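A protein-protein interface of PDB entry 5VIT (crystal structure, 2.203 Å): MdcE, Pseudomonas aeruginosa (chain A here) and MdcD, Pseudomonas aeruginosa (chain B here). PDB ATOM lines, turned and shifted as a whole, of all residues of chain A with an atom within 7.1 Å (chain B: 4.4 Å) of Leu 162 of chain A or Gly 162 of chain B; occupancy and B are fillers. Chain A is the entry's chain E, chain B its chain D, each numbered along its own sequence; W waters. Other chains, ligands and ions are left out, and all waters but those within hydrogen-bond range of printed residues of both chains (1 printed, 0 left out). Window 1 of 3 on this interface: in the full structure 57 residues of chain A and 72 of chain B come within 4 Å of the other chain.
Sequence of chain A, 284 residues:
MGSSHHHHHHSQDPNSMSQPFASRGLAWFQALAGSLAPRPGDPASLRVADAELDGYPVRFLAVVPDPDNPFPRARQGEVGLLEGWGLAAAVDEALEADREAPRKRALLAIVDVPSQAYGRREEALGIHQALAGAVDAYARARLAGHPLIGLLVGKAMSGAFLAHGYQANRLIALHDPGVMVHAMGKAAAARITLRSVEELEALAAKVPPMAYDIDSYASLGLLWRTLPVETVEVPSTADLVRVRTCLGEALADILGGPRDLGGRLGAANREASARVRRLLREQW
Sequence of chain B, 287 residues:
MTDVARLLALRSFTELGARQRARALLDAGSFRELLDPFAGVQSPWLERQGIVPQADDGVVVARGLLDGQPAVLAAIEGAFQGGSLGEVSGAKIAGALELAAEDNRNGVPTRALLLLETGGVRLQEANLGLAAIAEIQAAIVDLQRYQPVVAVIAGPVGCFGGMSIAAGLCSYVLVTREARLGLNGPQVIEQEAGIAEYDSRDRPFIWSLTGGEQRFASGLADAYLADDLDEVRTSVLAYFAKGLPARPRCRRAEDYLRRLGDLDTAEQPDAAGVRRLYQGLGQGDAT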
ATOM      1  N   VAL A 113     -13.417 -11.103 -13.606  1.00  0.00           N
ATOM      2  CA  VAL A 113     -13.888 -12.306 -14.255  1.00  0.00           C
ATOM      3  C   VAL A 113     -12.825 -13.392 -14.103  1.00  0.00           C
ATOM      4  O   VAL A 113     -11.667 -13.206 -14.502  1.00  0.00           O
ATOM      5  CB  VAL A 113     -14.223 -12.040 -15.743  1.00  0.00           C
ATOM      6  CG1 VAL A 113     -15.591 -11.370 -15.863  1.00  0.00           C
ATOM      7  CG2 VAL A 113     -13.159 -11.153 -16.388  1.00  0.00           C
ATOM      8  N   GLN A 116     -13.259 -17.460 -18.865  1.00  0.00           N
ATOM      9  CA  GLN A 116     -14.184 -18.174 -19.750  1.00  0.00           C
ATOM     10  C   GLN A 116     -14.914 -19.363 -19.130  1.00  0.00           C
ATOM     11  O   GLN A 116     -14.349 -20.092 -18.318  1.00  0.00           O
ATOM     12  CB  GLN A 116     -13.396 -18.638 -20.981  1.00  0.00           C
ATOM     13  CG  GLN A 116     -11.973 -18.041 -21.009  1.00  0.00           C
ATOM     14  CD  GLN A 116     -11.303 -18.465 -22.276  1.00  0.00           C
ATOM     15  OE1 GLN A 116     -11.523 -19.594 -22.763  1.00  0.00           O
ATOM     16  NE2 GLN A 116     -10.634 -17.545 -22.913  1.00  0.00           N
ATOM     17  N   LEU A 131     -18.747 -14.340 -27.263  1.00  0.00           N
ATOM     18  CA  LEU A 131     -17.749 -13.451 -26.690  1.00  0.00           C
ATOM     19  C   LEU A 131     -17.360 -12.451 -27.757  1.00  0.00           C
ATOM     20  O   LEU A 131     -17.101 -11.292 -27.448  1.00  0.00           O
ATOM     21  CB  LEU A 131     -16.550 -14.233 -26.149  1.00  0.00           C
ATOM     22  CG  LEU A 131     -16.721 -14.538 -24.653  1.00  0.00           C
ATOM     23  CD1 LEU A 131     -18.092 -15.159 -24.331  1.00  0.00           C
ATOM     24  CD2 LEU A 131     -15.579 -15.406 -24.105  1.00  0.00           C
ATOM     25  N   ALA A 134     -19.696  -9.447 -27.765  1.00  0.00           N
ATOM     26  CA  ALA A 134     -19.267  -8.488 -26.765  1.00  0.00           C
ATOM     27  C   ALA A 134     -18.129  -7.607 -27.284  1.00  0.00           C
ATOM     28  O   ALA A 134     -18.227  -6.376 -27.243  1.00  0.00           O
ATOM     29  CB  ALA A 134     -18.843  -9.208 -25.513  1.00  0.00           C
ATOM     30  N   VAL A 135     -17.057  -8.235 -27.771  1.00  0.00           N
ATOM     31  CA  VAL A 135     -15.894  -7.486 -28.241  1.00  0.00           C
ATOM     32  C   VAL A 135     -16.311  -6.515 -29.347  1.00  0.00           C
ATOM     33  O   VAL A 135     -15.885  -5.345 -29.367  1.00  0.00           O
ATOM     34  CB  VAL A 135     -14.767  -8.434 -28.764  1.00  0.00           C
ATOM     35  CG1 VAL A 135     -13.613  -7.635 -29.425  1.00  0.00           C
ATOM     36  CG2 VAL A 135     -14.227  -9.288 -27.651  1.00  0.00           C
ATOM     37  N   TYR A 138     -18.338  -3.426 -27.917  1.00  0.00           N
ATOM     38  CA  TYR A 138     -17.387  -2.540 -27.259  1.00  0.00           C
ATOM     39  C   TYR A 138     -16.528  -1.731 -28.233  1.00  0.00           C
ATOM     40  O   TYR A 138     -16.463  -0.500 -28.132  1.00  0.00           O
ATOM     41  CB  TYR A 138     -16.473  -3.344 -26.345  1.00  0.00           C
ATOM     42  CG  TYR A 138     -16.973  -3.546 -24.938  1.00  0.00           C
ATOM     43  CD1 TYR A 138     -17.234  -2.457 -24.107  1.00  0.00           C
ATOM     44  CD2 TYR A 138     -17.124  -4.827 -24.409  1.00  0.00           C
ATOM     45  CE1 TYR A 138     -17.665  -2.641 -22.799  1.00  0.00           C
ATOM     46  CE2 TYR A 138     -17.551  -5.020 -23.097  1.00  0.00           C
ATOM     47  CZ  TYR A 138     -17.828  -3.920 -22.301  1.00  0.00           C
ATOM     48  OH  TYR A 138     -18.240  -4.093 -21.000  1.00  0.00           O
ATOM     49  N   ALA A 156      -8.732 -10.619 -14.248  1.00  0.00           N
ATOM     50  CA  ALA A 156      -9.018 -10.263 -15.622  1.00  0.00           C
ATOM     51  C   ALA A 156      -8.339 -11.304 -16.489  1.00  0.00           C
ATOM     52  O   ALA A 156      -7.182 -11.131 -16.903  1.00  0.00           O
ATOM     53  CB  ALA A 156      -8.528  -8.843 -15.944  1.00  0.00           C
ATOM     54  N   MET A 157      -9.066 -12.387 -16.745  1.00  0.00           N
ATOM     55  CA  MET A 157      -8.488 -13.586 -17.327  1.00  0.00           C
ATOM     56  C   MET A 157      -8.969 -13.882 -18.728  1.00  0.00           C
ATOM     57  O   MET A 157     -10.182 -13.926 -18.991  1.00  0.00           O
ATOM     58  CB  MET A 157      -8.785 -14.801 -16.440  1.00  0.00           C
ATOM     59  CG  MET A 157      -8.282 -14.659 -15.011  1.00  0.00           C
ATOM     60  SD  MET A 157      -6.482 -14.581 -14.885  1.00  0.00           S
ATOM     61  CE  MET A 157      -6.063 -16.120 -15.701  1.00  0.00           C
ATOM     62  N   SER A 158      -8.003 -14.076 -19.623  1.00  0.00           N
ATOM     63  CA  SER A 158      -8.250 -14.752 -20.885  1.00  0.00           C
ATOM     64  C   SER A 158      -9.383 -14.101 -21.698  1.00  0.00           C
ATOM     65  O   SER A 158      -9.544 -12.873 -21.681  1.00  0.00           O
ATOM     66  CB  SER A 158      -8.557 -16.233 -20.582  1.00  0.00           C
ATOM     67  OG  SER A 158      -8.630 -17.022 -21.752  1.00  0.00           O
ATOM     68  N   GLY A 159     -10.181 -14.925 -22.375  1.00  0.00           N
ATOM     69  CA  GLY A 159     -11.248 -14.450 -23.240  1.00  0.00           C
ATOM     70  C   GLY A 159     -12.342 -13.704 -22.487  1.00  0.00           C
ATOM     71  O   GLY A 159     -13.062 -12.911 -23.088  1.00  0.00           O
ATOM     72  N   ALA A 160     -12.465 -13.953 -21.182  1.00  0.00           N
ATOM     73  CA  ALA A 160     -13.427 -13.218 -20.359  1.00  0.00           C
ATOM     74  C   ALA A 160     -13.021 -11.747 -20.341  1.00  0.00           C
ATOM     75  O   ALA A 160     -13.865 -10.859 -20.507  1.00  0.00           O
ATOM     76  CB  ALA A 160     -13.498 -13.787 -18.926  1.00  0.00           C
ATOM     77  N   PHE A 161     -11.723 -11.498 -20.155  1.00  0.00           N
ATOM     78  CA  PHE A 161     -11.201 -10.134 -20.180  1.00  0.00           C
ATOM     79  C   PHE A 161     -11.290  -9.575 -21.607  1.00  0.00           C
ATOM     80  O   PHE A 161     -11.694  -8.433 -21.789  1.00  0.00           O
ATOM     81  CB  PHE A 161      -9.760 -10.096 -19.651  1.00  0.00           C
ATOM     82  CG  PHE A 161      -9.180  -8.706 -19.517  1.00  0.00           C
ATOM     83  CD1 PHE A 161      -9.995  -7.595 -19.386  1.00  0.00           C
ATOM     84  CD2 PHE A 161      -7.801  -8.518 -19.530  1.00  0.00           C
ATOM     85  CE1 PHE A 161      -9.453  -6.323 -19.266  1.00  0.00           C
ATOM     86  CE2 PHE A 161      -7.243  -7.243 -19.417  1.00  0.00           C
ATOM     87  CZ  PHE A 161      -8.076  -6.142 -19.279  1.00  0.00           C
ATOM     88  N   LEU A 162     -10.932 -10.377 -22.610  1.00  0.00           N
ATOM     89  CA  LEU A 162     -11.073  -9.938 -23.991  1.00  0.00           C
ATOM     90  C   LEU A 162     -12.496  -9.436 -24.258  1.00  0.00           C
ATOM     91  O   LEU A 162     -12.668  -8.368 -24.829  1.00  0.00           O
ATOM     92  CB  LEU A 162     -10.729 -11.060 -24.976  1.00  0.00           C
ATOM     93  CG  LEU A 162      -9.263 -11.494 -25.135  1.00  0.00           C
ATOM     94  CD1 LEU A 162      -9.185 -12.786 -25.954  1.00  0.00           C
ATOM     95  CD2 LEU A 162      -8.372 -10.401 -25.747  1.00  0.00           C
ATOM     96  N   ALA A 163     -13.510 -10.193 -23.833  1.00  0.00           N
ATOM     97  CA  ALA A 163     -14.887  -9.811 -24.110  1.00  0.00           C
ATOM     98  C   ALA A 163     -15.349  -8.675 -23.201  1.00  0.00           C
ATOM     99  O   ALA A 163     -16.143  -7.836 -23.607  1.00  0.00           O
ATOM    100  CB  ALA A 163     -15.821 -11.014 -23.970  1.00  0.00           C
ATOM    101  N   HIS A 164     -14.860  -8.658 -21.966  1.00  0.00           N
ATOM    102  CA  HIS A 164     -15.260  -7.637 -21.013  1.00  0.00           C
ATOM    103  C   HIS A 164     -14.054  -6.852 -20.455  1.00  0.00           C
ATOM    104  O   HIS A 164     -13.414  -7.258 -19.489  1.00  0.00           O
ATOM    105  CB  HIS A 164     -16.068  -8.272 -19.871  1.00  0.00           C
ATOM    106  CG  HIS A 164     -16.507  -7.292 -18.828  1.00  0.00           C
ATOM    107  ND1 HIS A 164     -17.298  -6.202 -19.119  1.00  0.00           N
ATOM    108  CD2 HIS A 164     -16.240  -7.220 -17.500  1.00  0.00           C
ATOM    109  CE1 HIS A 164     -17.502  -5.503 -18.017  1.00  0.00           C
ATOM    110  NE2 HIS A 164     -16.870  -6.101 -17.018  1.00  0.00           N
ATOM    111  N   GLY A 165     -13.761  -5.714 -21.072  1.00  0.00           N
ATOM    112  CA  GLY A 165     -12.689  -4.858 -20.605  1.00  0.00           C
ATOM    113  C   GLY A 165     -11.583  -4.549 -21.611  1.00  0.00           C
ATOM    114  O   GLY A 165     -11.129  -3.405 -21.689  1.00  0.00           O
ATOM    115  N   TYR A 166     -11.129  -5.539 -22.377  1.00  0.00           N
ATOM    116  CA  TYR A 166      -9.835  -5.354 -23.039  1.00  0.00           C
ATOM    117  C   TYR A 166      -9.916  -4.414 -24.237  1.00  0.00           C
ATOM    118  O   TYR A 166      -8.881  -4.072 -24.795  1.00  0.00           O
ATOM    119  CB  TYR A 166      -9.223  -6.672 -23.522  1.00  0.00           C
ATOM    120  CG  TYR A 166      -7.760  -6.841 -23.120  1.00  0.00           C
ATOM    121  CD1 TYR A 166      -7.266  -8.090 -22.714  1.00  0.00           C
ATOM    122  CD2 TYR A 166      -6.914  -5.737 -22.990  1.00  0.00           C
ATOM    123  CE1 TYR A 166      -5.937  -8.246 -22.306  1.00  0.00           C
ATOM    124  CE2 TYR A 166      -5.609  -5.879 -22.540  1.00  0.00           C
ATOM    125  CZ  TYR A 166      -5.111  -7.123 -22.218  1.00  0.00           C
ATOM    126  OH  TYR A 166      -3.779  -7.200 -21.807  1.00  0.00           O
ATOM    127  N   GLN A 167     -11.117  -4.007 -24.651  1.00  0.00           N
ATOM    128  CA  GLN A 167     -11.208  -3.020 -25.719  1.00  0.00           C
ATOM    129  C   GLN A 167     -11.161  -1.579 -25.212  1.00  0.00           C
ATOM    130  O   GLN A 167     -11.395  -0.654 -25.993  1.00  0.00           O
ATOM    131  CB  GLN A 167     -12.480  -3.222 -26.550  1.00  0.00           C
ATOM    132  CG  GLN A 167     -12.476  -4.459 -27.428  1.00  0.00           C
ATOM    133  CD  GLN A 167     -11.351  -4.449 -28.444  1.00  0.00           C
ATOM    134  OE1 GLN A 167     -11.187  -3.494 -29.225  1.00  0.00           O
ATOM    135  NE2 GLN A 167     -10.561  -5.509 -28.436  1.00  0.00           N
ATOM    136  N   LEU B 130      -1.958 -12.253 -25.320  1.00  0.00           N
ATOM    137  CA  LEU B 130      -3.327 -11.841 -25.052  1.00  0.00           C
ATOM    138  C   LEU B 130      -3.524 -10.348 -25.384  1.00  0.00           C
ATOM    139  O   LEU B 130      -4.515  -9.973 -25.999  1.00  0.00           O
ATOM    140  CB  LEU B 130      -3.688 -12.136 -23.595  1.00  0.00           C
ATOM    141  CG  LEU B 130      -5.163 -12.072 -23.184  1.00  0.00           C
ATOM    142  CD1 LEU B 130      -6.004 -13.116 -23.919  1.00  0.00           C
ATOM    143  CD2 LEU B 130      -5.307 -12.234 -21.654  1.00  0.00           C
ATOM    144  N   ILE B 133      -3.844 -10.060 -29.162  1.00  0.00           N
ATOM    145  CA  ILE B 133      -5.124 -10.569 -29.636  1.00  0.00           C
ATOM    146  C   ILE B 133      -6.221  -9.504 -29.474  1.00  0.00           C
ATOM    147  O   ILE B 133      -7.051  -9.308 -30.368  1.00  0.00           O
ATOM    148  CB  ILE B 133      -5.497 -11.874 -28.883  1.00  0.00           C
ATOM    149  CG1 ILE B 133      -4.554 -13.003 -29.309  1.00  0.00           C
ATOM    150  CG2 ILE B 133      -6.936 -12.279 -29.154  1.00  0.00           C
ATOM    151  CD1 ILE B 133      -4.917 -14.369 -28.750  1.00  0.00           C
ATOM    152  N   ALA B 134      -6.186  -8.787 -28.354  1.00  0.00           N
ATOM    153  CA  ALA B 134      -7.063  -7.629 -28.162  1.00  0.00           C
ATOM    154  C   ALA B 134      -6.898  -6.602 -29.271  1.00  0.00           C
ATOM    155  O   ALA B 134      -7.890  -6.052 -29.744  1.00  0.00           O
ATOM    156  CB  ALA B 134      -6.812  -6.976 -26.798  1.00  0.00           C
ATOM    157  N   GLN B 137      -8.302  -8.065 -32.550  1.00  0.00           N
ATOM    158  CA  GLN B 137      -9.754  -7.937 -32.527  1.00  0.00           C
ATOM    159  C   GLN B 137     -10.197  -6.502 -32.807  1.00  0.00           C
ATOM    160  O   GLN B 137     -11.089  -6.276 -33.629  1.00  0.00           O
ATOM    161  CB  GLN B 137     -10.306  -8.416 -31.181  1.00  0.00           C
ATOM    162  CG  GLN B 137     -10.224  -9.920 -30.998  1.00  0.00           C
ATOM    163  CD  GLN B 137     -10.436 -10.349 -29.557  1.00  0.00           C
ATOM    164  OE1 GLN B 137     -10.495  -9.517 -28.652  1.00  0.00           O
ATOM    165  NE2 GLN B 137     -10.535 -11.659 -29.335  1.00  0.00           N
ATOM    166  N   PHE B 160      -8.519 -21.976 -32.037  1.00  0.00           N
ATOM    167  CA  PHE B 160      -8.978 -21.982 -30.652  1.00  0.00           C
ATOM    168  C   PHE B 160      -8.573 -20.733 -29.905  1.00  0.00           C
ATOM    169  O   PHE B 160      -7.768 -19.933 -30.399  1.00  0.00           O
ATOM    170  CB  PHE B 160      -8.440 -23.221 -29.914  1.00  0.00           C
ATOM    171  CG  PHE B 160      -9.019 -24.519 -30.427  1.00  0.00           C
ATOM    172  CD1 PHE B 160     -10.157 -25.071 -29.833  1.00  0.00           C
ATOM    173  CD2 PHE B 160      -8.455 -25.160 -31.529  1.00  0.00           C
ATOM    174  CE1 PHE B 160     -10.715 -26.253 -30.310  1.00  0.00           C
ATOM    175  CE2 PHE B 160      -8.998 -26.345 -32.007  1.00  0.00           C
ATOM    176  CZ  PHE B 160     -10.138 -26.893 -31.399  1.00  0.00           C
ATOM    177  N   GLY B 161      -9.127 -20.589 -28.701  1.00  0.00           N
ATOM    178  CA  GLY B 161      -8.735 -19.543 -27.782  1.00  0.00           C
ATOM    179  C   GLY B 161      -9.123 -18.149 -28.242  1.00  0.00           C
ATOM    180  O   GLY B 161     -10.154 -17.962 -28.907  1.00  0.00           O
ATOM    181  N   GLY B 162      -8.288 -17.173 -27.881  1.00  0.00           N
ATOM    182  CA  GLY B 162      -8.520 -15.773 -28.204  1.00  0.00           C
ATOM    183  C   GLY B 162      -8.823 -15.550 -29.670  1.00  0.00           C
ATOM    184  O   GLY B 162      -9.641 -14.707 -30.023  1.00  0.00           O
ATOM    185  N   MET B 163      -8.186 -16.329 -30.533  1.00  0.00           N
ATOM    186  CA  MET B 163      -8.366 -16.140 -31.959  1.00  0.00           C
ATOM    187  C   MET B 163      -9.654 -16.767 -32.493  1.00  0.00           C
ATOM    188  O   MET B 163     -10.056 -16.484 -33.622  1.00  0.00           O
ATOM    189  CB  MET B 163      -7.159 -16.686 -32.715  1.00  0.00           C
ATOM    190  CG  MET B 163      -5.908 -15.861 -32.496  1.00  0.00           C
ATOM    191  SD  MET B 163      -6.146 -14.140 -32.997  1.00  0.00           S
ATOM    192  CE  MET B 163      -6.266 -14.329 -34.768  1.00  0.00           C
ATOM    193  N   SER B 164     -10.313 -17.608 -31.697  1.00  0.00           N
ATOM    194  CA  SER B 164     -11.637 -18.058 -32.117  1.00  0.00           C
ATOM    195  C   SER B 164     -12.604 -16.883 -31.952  1.00  0.00           C
ATOM    196  O   SER B 164     -13.494 -16.699 -32.774  1.00  0.00           O
ATOM    197  CB  SER B 164     -12.111 -19.286 -31.338  1.00  0.00           C
ATOM    198  OG  SER B 164     -12.338 -19.007 -29.974  1.00  0.00           O
ATOM    199  N   ILE B 165     -12.397 -16.075 -30.912  1.00  0.00           N
ATOM    200  CA  ILE B 165     -13.193 -14.869 -30.731  1.00  0.00           C
ATOM    201  C   ILE B 165     -12.921 -13.895 -31.878  1.00  0.00           C
ATOM    202  O   ILE B 165     -13.830 -13.224 -32.379  1.00  0.00           O
ATOM    203  CB  ILE B 165     -12.905 -14.209 -29.395  1.00  0.00           C
ATOM    204  CG1 ILE B 165     -13.171 -15.197 -28.267  1.00  0.00           C
ATOM    205  CG2 ILE B 165     -13.779 -12.974 -29.211  1.00  0.00           C
ATOM    206  CD1 ILE B 165     -12.867 -14.617 -26.881  1.00  0.00           C
ATOM    207  N   ALA B 166     -11.677 -13.856 -32.334  1.00  0.00           N
ATOM    208  CA  ALA B 166     -11.337 -12.992 -33.446  1.00  0.00           C
ATOM    209  C   ALA B 166     -12.059 -13.494 -34.693  1.00  0.00           C
ATOM    210  O   ALA B 166     -12.530 -12.701 -35.528  1.00  0.00           O
ATOM    211  CB  ALA B 166      -9.811 -12.949 -33.666  1.00  0.00           C
HETATM  212  O   HOH W   1     -10.724  -7.604 -26.673  1.00  0.00           O
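NE2 of Gln 167 of chain A is in hydrogen-bond range of O of Ala 134 of chain B (3.0 Å).
The backbone carbonyl oxygen of Gly 162 of chain B lies within hydrogen-bond range of the side-chain amide nitrogen of Gln 137 of chain B, 3.3 Å away. The backbone NH (N) of Gly 159 of chain A lies close to the side-chain amide nitrogen (NE2) of Gln 116 of chain A, 2.7 Å away. The backbone carbonyl oxygen of Phe 161 of chain A is in hydrogen-bond range of the backbone NH of Tyr 166 of chain A (3.0 Å).
Ile 165 of chain B touches Leu 131 of chain A (CD1 to CB, 3.8 Å). Val 135 of chain A touches Gln 137 of chain B. CD2 of Leu 130 of chain B touches N of Ser 158 of chain A, 3.8 Å away. CA of Gly 159 of chain A touches CD1 of Ile 165 of chain B, 3.99 Å away. Leu 162 of chain A touches Leu 130 of chain B. Ile 133 of chain B touches Leu 162 of chain A. Leu 162 of chain A touches Ala 134 of chain B. Gln 137 of chain B touches Leu 162 of chain A. Gly 162 of chain B touches Leu 162 of chain A (CA to CD1, 3.8 Å). CB of Ala 134 of chain B touches CG of Tyr 166 of chain A, at 3.8 Å.
Of the printed residues of chain B, Val 135 of chain A touches Gln 137. Of chain B, only Leu 130, Ile 133, Ala 134, Gln 137 and Gly 162 come within 4 Å of Leu 162 of chain A. Of the printed residues of chain B, Gln 167 of chain A touches Ala 134 (3.0 Å). Of the printed residues of chain A, Leu 130 of chain B touches Ser 158 and Leu 162. Of the printed residues of chain A, Gln 137 of chain B touches Val 135 (3.7 Å) and Leu 162 (3.7 Å). Gly 162 of chain B touches one residue of chain A. Of the printed residues of chain A, Ile 165 of chain B touches Leu 131 and Gly 159. The nearest residue of chain A that does not touch Gly 162 of chain B is Gln 116 of chain A (5.5 Å).
Of the 18 printed residues of chain A, 7 touch a printed residue of chain B. Printed residues of chain A that touch a printed residue of chain B: Leu 131, Val 135, Ser 158, Gly 159, Leu 162, Tyr 166 and Gln 167. Hydrophobic or aromatic side chains of chain A within 4 Å of the printed part of chain B: Leu 131, Val 135, Leu 162 and Tyr 166. Of the 11 printed residues of chain B, 6 touch a printed residue of chain A. Printed residues of chain B that touch a printed residue of chain A: Leu 130, Ile 133, Ala 134, Gln 137, Gly 162 and Ile 165.
Water W1 lies within hydrogen-bond range of the side-chain amide nitrogen of Gln 167 of chain A (2.7 Å), the side-chain amide oxygen of Gln 137 of chain B (2.8 Å) and the backbone carbonyl oxygen of Leu 162 of chain A (2.8 Å).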
